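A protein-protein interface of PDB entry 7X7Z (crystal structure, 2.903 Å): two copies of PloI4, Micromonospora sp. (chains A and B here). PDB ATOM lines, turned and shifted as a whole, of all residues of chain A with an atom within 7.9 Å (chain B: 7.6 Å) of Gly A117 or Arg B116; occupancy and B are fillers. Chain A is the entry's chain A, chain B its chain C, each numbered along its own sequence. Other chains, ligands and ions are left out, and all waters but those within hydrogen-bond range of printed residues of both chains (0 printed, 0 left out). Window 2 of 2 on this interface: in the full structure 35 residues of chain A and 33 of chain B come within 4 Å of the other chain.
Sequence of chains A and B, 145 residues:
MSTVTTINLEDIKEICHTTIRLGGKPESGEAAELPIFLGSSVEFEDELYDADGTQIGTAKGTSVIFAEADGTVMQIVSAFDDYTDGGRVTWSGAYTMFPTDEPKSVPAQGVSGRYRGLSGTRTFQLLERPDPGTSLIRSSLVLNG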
ATOM      1  N   THR A   5     -24.362   7.706 -20.077  1.00  0.00           N
ATOM      2  CA  THR A   5     -23.313   7.455 -19.097  1.00  0.00           C
ATOM      3  C   THR A   5     -23.913   6.913 -17.805  1.00  0.00           C
ATOM      4  O   THR A   5     -24.959   7.382 -17.345  1.00  0.00           O
ATOM      5  CB  THR A   5     -22.529   8.744 -18.823  1.00  0.00           C
ATOM      6  OG1 THR A   5     -21.751   9.086 -19.977  1.00  0.00           O
ATOM      7  CG2 THR A   5     -21.599   8.587 -17.621  1.00  0.00           C
ATOM      8  N   ARG A  88     -19.035  16.428  -6.844  1.00  0.00           N
ATOM      9  CA  ARG A  88     -19.918  16.396  -5.693  1.00  0.00           C
ATOM     10  C   ARG A  88     -21.250  15.785  -6.097  1.00  0.00           C
ATOM     11  O   ARG A  88     -21.784  16.086  -7.170  1.00  0.00           O
ATOM     12  CB  ARG A  88     -20.122  17.804  -5.137  1.00  0.00           C
ATOM     13  CG  ARG A  88     -21.281  17.921  -4.174  1.00  0.00           C
ATOM     14  CD  ARG A  88     -21.582  19.371  -3.857  1.00  0.00           C
ATOM     15  NE  ARG A  88     -20.615  19.933  -2.919  1.00  0.00           N
ATOM     16  CZ  ARG A  88     -20.923  20.807  -1.966  1.00  0.00           C
ATOM     17  NH1 ARG A  88     -22.176  21.221  -1.822  1.00  0.00           N
ATOM     18  NH2 ARG A  88     -19.980  21.267  -1.157  1.00  0.00           N
ATOM     19  N   GLN A 109     -28.025  13.222  -6.796  1.00  0.00           N
ATOM     20  CA  GLN A 109     -27.856  14.093  -7.954  1.00  0.00           C
ATOM     21  C   GLN A 109     -26.396  14.502  -8.066  1.00  0.00           C
ATOM     22  O   GLN A 109     -25.840  15.087  -7.130  1.00  0.00           O
ATOM     23  CB  GLN A 109     -28.746  15.338  -7.849  1.00  0.00           C
ATOM     24  CG  GLN A 109     -30.201  15.057  -7.510  1.00  0.00           C
ATOM     25  CD  GLN A 109     -30.441  14.938  -6.017  1.00  0.00           C
ATOM     26  OE1 GLN A 109     -29.714  15.520  -5.211  1.00  0.00           O
ATOM     27  NE2 GLN A 109     -31.461  14.177  -5.642  1.00  0.00           N
ATOM     28  N   GLY A 110     -25.781  14.201  -9.207  1.00  0.00           N
ATOM     29  CA  GLY A 110     -24.427  14.659  -9.471  1.00  0.00           C
ATOM     30  C   GLY A 110     -24.444  16.102  -9.937  1.00  0.00           C
ATOM     31  O   GLY A 110     -25.154  16.453 -10.886  1.00  0.00           O
ATOM     32  N   VAL A 111     -23.661  16.944  -9.266  1.00  0.00           N
ATOM     33  CA  VAL A 111     -23.713  18.381  -9.503  1.00  0.00           C
ATOM     34  C   VAL A 111     -22.409  18.953 -10.041  1.00  0.00           C
ATOM     35  O   VAL A 111     -22.419  20.077 -10.567  1.00  0.00           O
ATOM     36  CB  VAL A 111     -24.133  19.133  -8.224  1.00  0.00           C
ATOM     37  CG1 VAL A 111     -25.302  18.429  -7.566  1.00  0.00           C
ATOM     38  CG2 VAL A 111     -22.964  19.246  -7.260  1.00  0.00           C
ATOM     39  N   SER A 112     -21.290  18.244  -9.936  1.00  0.00           N
ATOM     40  CA  SER A 112     -20.014  18.759 -10.409  1.00  0.00           C
ATOM     41  C   SER A 112     -19.131  17.593 -10.827  1.00  0.00           C
ATOM     42  O   SER A 112     -19.435  16.427 -10.561  1.00  0.00           O
ATOM     43  CB  SER A 112     -19.325  19.611  -9.336  1.00  0.00           C
ATOM     44  OG  SER A 112     -18.649  18.797  -8.395  1.00  0.00           O
ATOM     45  N   GLY A 113     -18.025  17.923 -11.492  1.00  0.00           N
ATOM     46  CA  GLY A 113     -17.093  16.903 -11.927  1.00  0.00           C
ATOM     47  C   GLY A 113     -17.690  15.990 -12.987  1.00  0.00           C
ATOM     48  O   GLY A 113     -18.649  16.331 -13.685  1.00  0.00           O
ATOM     49  N   ARG A 114     -17.102  14.796 -13.094  1.00  0.00           N
ATOM     50  CA  ARG A 114     -17.578  13.816 -14.063  1.00  0.00           C
ATOM     51  C   ARG A 114     -18.936  13.233 -13.692  1.00  0.00           C
ATOM     52  O   ARG A 114     -19.498  12.465 -14.481  1.00  0.00           O
ATOM     53  CB  ARG A 114     -16.538  12.701 -14.228  1.00  0.00           C
ATOM     54  CG  ARG A 114     -16.683  11.533 -13.266  1.00  0.00           C
ATOM     55  CD  ARG A 114     -15.684  10.429 -13.595  1.00  0.00           C
ATOM     56  NE  ARG A 114     -16.200   9.097 -13.288  1.00  0.00           N
ATOM     57  CZ  ARG A 114     -15.947   8.436 -12.163  1.00  0.00           C
ATOM     58  NH1 ARG A 114     -15.181   8.981 -11.229  1.00  0.00           N
ATOM     59  NH2 ARG A 114     -16.460   7.227 -11.972  1.00  0.00           N
ATOM     60  N   TYR A 115     -19.480  13.582 -12.526  1.00  0.00           N
ATOM     61  CA  TYR A 115     -20.837  13.203 -12.160  1.00  0.00           C
ATOM     62  C   TYR A 115     -21.854  14.293 -12.471  1.00  0.00           C
ATOM     63  O   TYR A 115     -23.053  14.069 -12.274  1.00  0.00           O
ATOM     64  CB  TYR A 115     -20.925  12.851 -10.666  1.00  0.00           C
ATOM     65  CG  TYR A 115     -20.011  11.730 -10.216  1.00  0.00           C
ATOM     66  CD1 TYR A 115     -19.444  10.854 -11.130  1.00  0.00           C
ATOM     67  CD2 TYR A 115     -19.725  11.541  -8.871  1.00  0.00           C
ATOM     68  CE1 TYR A 115     -18.607   9.836 -10.715  1.00  0.00           C
ATOM     69  CE2 TYR A 115     -18.890  10.530  -8.450  1.00  0.00           C
ATOM     70  CZ  TYR A 115     -18.335   9.677  -9.374  1.00  0.00           C
ATOM     71  OH  TYR A 115     -17.506   8.663  -8.953  1.00  0.00           O
ATOM     72  N   ARG A 116     -21.405  15.456 -12.941  1.00  0.00           N
ATOM     73  CA  ARG A 116     -22.305  16.559 -13.260  1.00  0.00           C
ATOM     74  C   ARG A 116     -23.356  16.122 -14.273  1.00  0.00           C
ATOM     75  O   ARG A 116     -23.029  15.567 -15.325  1.00  0.00           O
ATOM     76  CB  ARG A 116     -21.504  17.744 -13.809  1.00  0.00           C
ATOM     77  CG  ARG A 116     -22.210  19.090 -13.725  1.00  0.00           C
ATOM     78  CD  ARG A 116     -21.346  20.217 -14.290  1.00  0.00           C
ATOM     79  NE  ARG A 116     -20.406  20.754 -13.306  1.00  0.00           N
ATOM     80  CZ  ARG A 116     -19.083  20.620 -13.372  1.00  0.00           C
ATOM     81  NH1 ARG A 116     -18.315  21.145 -12.428  1.00  0.00           N
ATOM     82  NH2 ARG A 116     -18.524  19.957 -14.378  1.00  0.00           N
ATOM     83  N   GLY A 117     -24.623  16.367 -13.944  1.00  0.00           N
ATOM     84  CA  GLY A 117     -25.723  16.036 -14.824  1.00  0.00           C
ATOM     85  C   GLY A 117     -26.283  14.639 -14.671  1.00  0.00           C
ATOM     86  O   GLY A 117     -27.280  14.313 -15.329  1.00  0.00           O
ATOM     87  N   LEU A 118     -25.681  13.805 -13.832  1.00  0.00           N
ATOM     88  CA  LEU A 118     -26.149  12.445 -13.614  1.00  0.00           C
ATOM     89  C   LEU A 118     -26.972  12.366 -12.334  1.00  0.00           C
ATOM     90  O   LEU A 118     -26.705  13.068 -11.356  1.00  0.00           O
ATOM     91  CB  LEU A 118     -24.972  11.473 -13.543  1.00  0.00           C
ATOM     92  CG  LEU A 118     -24.015  11.529 -14.735  1.00  0.00           C
ATOM     93  CD1 LEU A 118     -22.886  10.534 -14.559  1.00  0.00           C
ATOM     94  CD2 LEU A 118     -24.761  11.270 -16.034  1.00  0.00           C
ATOM     95  N   SER A 119     -27.979  11.497 -12.351  1.00  0.00           N
ATOM     96  CA  SER A 119     -28.898  11.351 -11.233  1.00  0.00           C
ATOM     97  C   SER A 119     -29.207   9.879 -11.008  1.00  0.00           C
ATOM     98  O   SER A 119     -29.160   9.068 -11.936  1.00  0.00           O
ATOM     99  CB  SER A 119     -30.199  12.121 -11.473  1.00  0.00           C
ATOM    100  OG  SER A 119     -31.069  11.405 -12.331  1.00  0.00           O
ATOM    101  N   GLY A 120     -29.532   9.545  -9.761  1.00  0.00           N
ATOM    102  CA  GLY A 120     -29.866   8.179  -9.413  1.00  0.00           C
ATOM    103  C   GLY A 120     -30.208   7.982  -7.952  1.00  0.00           C
ATOM    104  O   GLY A 120     -31.006   8.734  -7.386  1.00  0.00           O
ATOM    105  N   LEU A 143     -25.750   6.392 -10.625  1.00  0.00           N
ATOM    106  CA  LEU A 143     -26.086   7.621 -11.331  1.00  0.00           C
ATOM    107  C   LEU A 143     -26.253   7.320 -12.812  1.00  0.00           C
ATOM    108  O   LEU A 143     -25.524   6.495 -13.371  1.00  0.00           O
ATOM    109  CB  LEU A 143     -25.008   8.695 -11.129  1.00  0.00           C
ATOM    110  CG  LEU A 143     -24.830   9.233  -9.707  1.00  0.00           C
ATOM    111  CD1 LEU A 143     -23.698  10.247  -9.654  1.00  0.00           C
ATOM    112  CD2 LEU A 143     -26.124   9.844  -9.191  1.00  0.00           C
ATOM    113  N   ASN A 144     -27.212   7.994 -13.446  1.00  0.00           N
ATOM    114  CA  ASN A 144     -27.514   7.766 -14.850  1.00  0.00           C
ATOM    115  C   ASN A 144     -27.772   9.095 -15.542  1.00  0.00           C
ATOM    116  O   ASN A 144     -28.083  10.104 -14.903  1.00  0.00           O
ATOM    117  CB  ASN A 144     -28.726   6.841 -15.025  1.00  0.00           C
ATOM    118  CG  ASN A 144     -28.342   5.378 -15.051  1.00  0.00           C
ATOM    119  OD1 ASN A 144     -27.746   4.897 -16.014  1.00  0.00           O
ATOM    120  ND2 ASN A 144     -28.679   4.661 -13.986  1.00  0.00           N
ATOM    121  N   GLY A 145     -27.641   9.081 -16.865  1.00  0.00           N
ATOM    122  CA  GLY A 145     -27.888  10.259 -17.676  1.00  0.00           C
ATOM    123  C   GLY A 145     -29.258  10.247 -18.326  1.00  0.00           C
ATOM    124  O   GLY A 145     -30.242   9.821 -17.721  1.00  0.00           O
ATOM    125  OXT GLY A 145     -29.420  10.663 -19.473  1.00  0.00           O
ATOM    126  N   GLY B  86     -38.361  23.854 -18.175  1.00  0.00           N
ATOM    127  CA  GLY B  86     -38.475  22.410 -18.251  1.00  0.00           C
ATOM    128  C   GLY B  86     -37.552  21.624 -17.343  1.00  0.00           C
ATOM    129  O   GLY B  86     -36.398  21.999 -17.132  1.00  0.00           O
ATOM    130  N   GLY B  87     -38.071  20.531 -16.804  1.00  0.00           N
ATOM    131  CA  GLY B  87     -37.279  19.577 -16.057  1.00  0.00           C
ATOM    132  C   GLY B  87     -37.537  19.653 -14.562  1.00  0.00           C
ATOM    133  O   GLY B  87     -38.223  20.539 -14.051  1.00  0.00           O
ATOM    134  N   ARG B  88     -36.958  18.679 -13.865  1.00  0.00           N
ATOM    135  CA  ARG B  88     -37.039  18.593 -12.416  1.00  0.00           C
ATOM    136  C   ARG B  88     -35.829  19.275 -11.790  1.00  0.00           C
ATOM    137  O   ARG B  88     -34.711  19.178 -12.305  1.00  0.00           O
ATOM    138  CB  ARG B  88     -37.112  17.131 -11.972  1.00  0.00           C
ATOM    139  CG  ARG B  88     -36.979  16.909 -10.472  1.00  0.00           C
ATOM    140  CD  ARG B  88     -37.084  15.434 -10.121  1.00  0.00           C
ATOM    141  NE  ARG B  88     -38.372  14.876 -10.518  1.00  0.00           N
ATOM    142  CZ  ARG B  88     -39.104  14.069  -9.758  1.00  0.00           C
ATOM    143  NH1 ARG B  88     -38.675  13.724  -8.551  1.00  0.00           N
ATOM    144  NH2 ARG B  88     -40.266  13.611 -10.201  1.00  0.00           N
ATOM    145  N   VAL B  89     -36.062  19.975 -10.684  1.00  0.00           N
ATOM    146  CA  VAL B  89     -35.007  20.652  -9.940  1.00  0.00           C
ATOM    147  C   VAL B  89     -35.179  20.286  -8.473  1.00  0.00           C
ATOM    148  O   VAL B  89     -36.157  20.697  -7.839  1.00  0.00           O
ATOM    149  CB  VAL B  89     -35.041  22.175 -10.130  1.00  0.00           C
ATOM    150  CG1 VAL B  89     -34.139  22.860  -9.114  1.00  0.00           C
ATOM    151  CG2 VAL B  89     -34.620  22.534 -11.541  1.00  0.00           C
ATOM    152  N   GLN B 109     -30.458  21.814  -7.430  1.00  0.00           N
ATOM    153  CA  GLN B 109     -29.744  21.077  -8.467  1.00  0.00           C
ATOM    154  C   GLN B 109     -30.703  20.749  -9.600  1.00  0.00           C
ATOM    155  O   GLN B 109     -31.714  20.073  -9.383  1.00  0.00           O
ATOM    156  CB  GLN B 109     -29.125  19.791  -7.907  1.00  0.00           C
ATOM    157  CG  GLN B 109     -28.320  19.979  -6.630  1.00  0.00           C
ATOM    158  CD  GLN B 109     -29.173  19.923  -5.379  1.00  0.00           C
ATOM    159  OE1 GLN B 109     -30.112  19.134  -5.288  1.00  0.00           O
ATOM    160  NE2 GLN B 109     -28.846  20.764  -4.405  1.00  0.00           N
ATOM    161  N   GLY B 110     -30.387  21.227 -10.802  1.00  0.00           N
ATOM    162  CA  GLY B 110     -31.125  20.813 -11.985  1.00  0.00           C
ATOM    163  C   GLY B 110     -30.754  19.389 -12.369  1.00  0.00           C
ATOM    164  O   GLY B 110     -29.581  19.016 -12.403  1.00  0.00           O
ATOM    165  N   VAL B 111     -31.775  18.588 -12.670  1.00  0.00           N
ATOM    166  CA  VAL B 111     -31.586  17.143 -12.693  1.00  0.00           C
ATOM    167  C   VAL B 111     -32.174  16.506 -13.949  1.00  0.00           C
ATOM    168  O   VAL B 111     -31.930  15.326 -14.225  1.00  0.00           O
ATOM    169  CB  VAL B 111     -32.189  16.514 -11.423  1.00  0.00           C
ATOM    170  CG1 VAL B 111     -33.678  16.252 -11.599  1.00  0.00           C
ATOM    171  CG2 VAL B 111     -31.442  15.254 -11.048  1.00  0.00           C
ATOM    172  N   SER B 112     -32.944  17.270 -14.722  1.00  0.00           N
ATOM    173  CA  SER B 112     -33.545  16.733 -15.937  1.00  0.00           C
ATOM    174  C   SER B 112     -34.023  17.885 -16.808  1.00  0.00           C
ATOM    175  O   SER B 112     -34.177  19.017 -16.344  1.00  0.00           O
ATOM    176  CB  SER B 112     -34.706  15.784 -15.622  1.00  0.00           C
ATOM    177  OG  SER B 112     -35.841  16.498 -15.164  1.00  0.00           O
ATOM    178  N   GLY B 113     -34.251  17.575 -18.085  1.00  0.00           N
ATOM    179  CA  GLY B 113     -34.797  18.551 -19.008  1.00  0.00           C
ATOM    180  C   GLY B 113     -33.835  19.689 -19.303  1.00  0.00           C
ATOM    181  O   GLY B 113     -32.615  19.513 -19.382  1.00  0.00           O
ATOM    182  N   ARG B 114     -34.410  20.884 -19.476  1.00  0.00           N
ATOM    183  CA  ARG B 114     -33.612  22.071 -19.769  1.00  0.00           C
ATOM    184  C   ARG B 114     -32.598  22.347 -18.665  1.00  0.00           C
ATOM    185  O   ARG B 114     -31.468  22.769 -18.940  1.00  0.00           O
ATOM    186  CB  ARG B 114     -34.532  23.279 -19.956  1.00  0.00           C
ATOM    187  CG  ARG B 114     -34.163  24.198 -21.110  1.00  0.00           C
ATOM    188  CD  ARG B 114     -35.326  25.111 -21.484  1.00  0.00           C
ATOM    189  NE  ARG B 114     -35.856  25.848 -20.338  1.00  0.00           N
ATOM    190  CZ  ARG B 114     -35.344  26.988 -19.881  1.00  0.00           C
ATOM    191  NH1 ARG B 114     -34.288  27.526 -20.474  1.00  0.00           N
ATOM    192  NH2 ARG B 114     -35.890  27.593 -18.833  1.00  0.00           N
ATOM    193  N   TYR B 115     -32.977  22.106 -17.415  1.00  0.00           N
ATOM    194  CA  TYR B 115     -32.182  22.490 -16.258  1.00  0.00           C
ATOM    195  C   TYR B 115     -31.130  21.458 -15.870  1.00  0.00           C
ATOM    196  O   TYR B 115     -30.382  21.694 -14.915  1.00  0.00           O
ATOM    197  CB  TYR B 115     -33.102  22.750 -15.059  1.00  0.00           C
ATOM    198  CG  TYR B 115     -34.124  23.840 -15.295  1.00  0.00           C
ATOM    199  CD1 TYR B 115     -35.371  23.790 -14.689  1.00  0.00           C
ATOM    200  CD2 TYR B 115     -33.841  24.920 -16.121  1.00  0.00           C
ATOM    201  CE1 TYR B 115     -36.308  24.782 -14.898  1.00  0.00           C
ATOM    202  CE2 TYR B 115     -34.771  25.916 -16.335  1.00  0.00           C
ATOM    203  CZ  TYR B 115     -36.003  25.843 -15.721  1.00  0.00           C
ATOM    204  OH  TYR B 115     -36.933  26.835 -15.934  1.00  0.00           O
ATOM    205  N   ARG B 116     -31.050  20.331 -16.578  1.00  0.00           N
ATOM    206  CA  ARG B 116     -30.112  19.277 -16.208  1.00  0.00           C
ATOM    207  C   ARG B 116     -28.678  19.789 -16.241  1.00  0.00           C
ATOM    208  O   ARG B 116     -28.244  20.393 -17.226  1.00  0.00           O
ATOM    209  CB  ARG B 116     -30.265  18.079 -17.147  1.00  0.00           C
ATOM    210  CG  ARG B 116     -29.294  16.939 -16.859  1.00  0.00           C
ATOM    211  CD  ARG B 116     -29.399  15.833 -17.900  1.00  0.00           C
ATOM    212  NE  ARG B 116     -30.470  14.885 -17.599  1.00  0.00           N
ATOM    213  CZ  ARG B 116     -31.579  14.750 -18.323  1.00  0.00           C
ATOM    214  NH1 ARG B 116     -32.497  13.860 -17.971  1.00  0.00           N
ATOM    215  NH2 ARG B 116     -31.771  15.502 -19.399  1.00  0.00           N
ATOM    216  N   GLY B 117     -27.945  19.551 -15.154  1.00  0.00           N
ATOM    217  CA  GLY B 117     -26.549  19.909 -15.052  1.00  0.00           C
ATOM    218  C   GLY B 117     -26.277  21.231 -14.363  1.00  0.00           C
ATOM    219  O   GLY B 117     -25.129  21.489 -13.984  1.00  0.00           O
ATOM    220  N   LEU B 118     -27.294  22.070 -14.191  1.00  0.00           N
ATOM    221  CA  LEU B 118     -27.122  23.377 -13.573  1.00  0.00           C
ATOM    222  C   LEU B 118     -27.320  23.273 -12.065  1.00  0.00           C
ATOM    223  O   LEU B 118     -28.284  22.659 -11.598  1.00  0.00           O
ATOM    224  CB  LEU B 118     -28.103  24.388 -14.166  1.00  0.00           C
ATOM    225  CG  LEU B 118     -28.204  24.434 -15.691  1.00  0.00           C
ATOM    226  CD1 LEU B 118     -29.287  25.408 -16.120  1.00  0.00           C
ATOM    227  CD2 LEU B 118     -26.864  24.812 -16.305  1.00  0.00           C
ATOM    228  N   SER B 119     -26.398  23.862 -11.314  1.00  0.00           N
ATOM    229  CA  SER B 119     -26.488  23.941  -9.865  1.00  0.00           C
ATOM    230  C   SER B 119     -26.775  25.377  -9.452  1.00  0.00           C
ATOM    231  O   SER B 119     -26.471  26.326 -10.180  1.00  0.00           O
ATOM    232  CB  SER B 119     -25.197  23.444  -9.203  1.00  0.00           C
ATOM    233  OG  SER B 119     -24.354  24.527  -8.843  1.00  0.00           O
ATOM    234  N   LEU B 143     -30.027  29.120 -11.275  1.00  0.00           N
ATOM    235  CA  LEU B 143     -29.202  27.980 -11.641  1.00  0.00           C
ATOM    236  C   LEU B 143     -28.206  28.402 -12.708  1.00  0.00           C
ATOM    237  O   LEU B 143     -28.564  29.106 -13.656  1.00  0.00           O
ATOM    238  CB  LEU B 143     -30.051  26.811 -12.162  1.00  0.00           C
ATOM    239  CG  LEU B 143     -31.009  26.108 -11.199  1.00  0.00           C
ATOM    240  CD1 LEU B 143     -31.874  25.114 -11.958  1.00  0.00           C
ATOM    241  CD2 LEU B 143     -30.246  25.410 -10.087  1.00  0.00           C
ATOM    242  N   GLY B 145     -24.326  26.890 -14.784  1.00  0.00           N
ATOM    243  CA  GLY B 145     -23.437  25.775 -15.049  1.00  0.00           C
ATOM    244  C   GLY B 145     -22.520  26.039 -16.227  1.00  0.00           C
ATOM    245  O   GLY B 145     -22.930  26.634 -17.224  1.00  0.00           O
ATOM    246  OXT GLY B 145     -21.346  25.666 -16.215  1.00  0.00           O
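O of Ser A119 is in hydrogen-bond range of N of Asn A144.
N of Gly B117 lies within hydrogen-bond range of O of Gly B110, at 3.2 Å.
The backbone NH of Gly A117 lies within hydrogen-bond range of the backbone carbonyl oxygen of Gly A110, 3.1 Å away.
The backbone carbonyl oxygen of Arg B88 is in hydrogen-bond range of the backbone NH of Val B111, 3.0 Å away.
The backbone NH of Val A111 sits at hydrogen-bond distance from the backbone carbonyl oxygen of Arg A88 (2.9 Å).
The backbone carbonyl oxygen (O) of Val A111 sits close to the guanidinium group (NE) of Arg A116, at 3.5 Å.
Among the printed residues, merely in contact across the chains: Ser A119 with Val B111 (3.4 Å), Val A111 with Gln B109 (3.5 Å), Gln A109 with Gln B109 (3.6 Å), Gly A117 with Arg B116 (3.6 Å), Gln A109 with Val B111 (3.8 Å), Arg A116 with Gly B117 (3.8 Å) and Gly A117 with Gly B117 (3.97 Å).
Gly A117 touches just these residues of chain B: Arg B116 (3.6 Å) and Gly B117 (3.97 Å).
Arg B116 touches just one residue of chain A: Gly A117.
Printed residues of chain A within 4 Å of Gln B109: Gln A109 and Val A111.
Printed residues of chain B within 4 Å of Ser A119: Val B111 (3.4 Å).
Leu A118 touches none of the printed residues of chain B.
The nearest residue of chain B that does not touch Gly A117 is Val B111 (4.9 Å).
The nearest residue of chain A that does not touch Arg B116 is Gly A145 (4.6 Å).
Of the 17 printed residues of chain A, 5 touch a printed residue of chain B.
Printed residues of chain A that touch a printed residue of chain B: Gln A109, Val A111, Arg A116, Gly A117 and Ser A119.
Among the printed residues, no Asp or Glu carboxylate lies within 4 Å of a Lys or Arg side-chain nitrogen of the other chain.
Gln A109 touches Val B111, and with the chains exchanged Val A111 touches Gln B109.
Arg A116 touches Gly B117, and with the chains exchanged Gly A117 touches Arg B116.
Gly B117 touches its own counterpart, Gly A117.
Ser A119 touches Val B111, but with the chains exchanged Val A111 does not touch Ser B119 (4.5 Å).
Positions printed for both chains: 88, 109, 110, 111, 112, 113, 114, 115, 116, 117, 118, 119, 143 and 145.
Of the 7 pairs that touch across the chains among the printed residues, 6 have their exchanged pair printed and touching as well.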
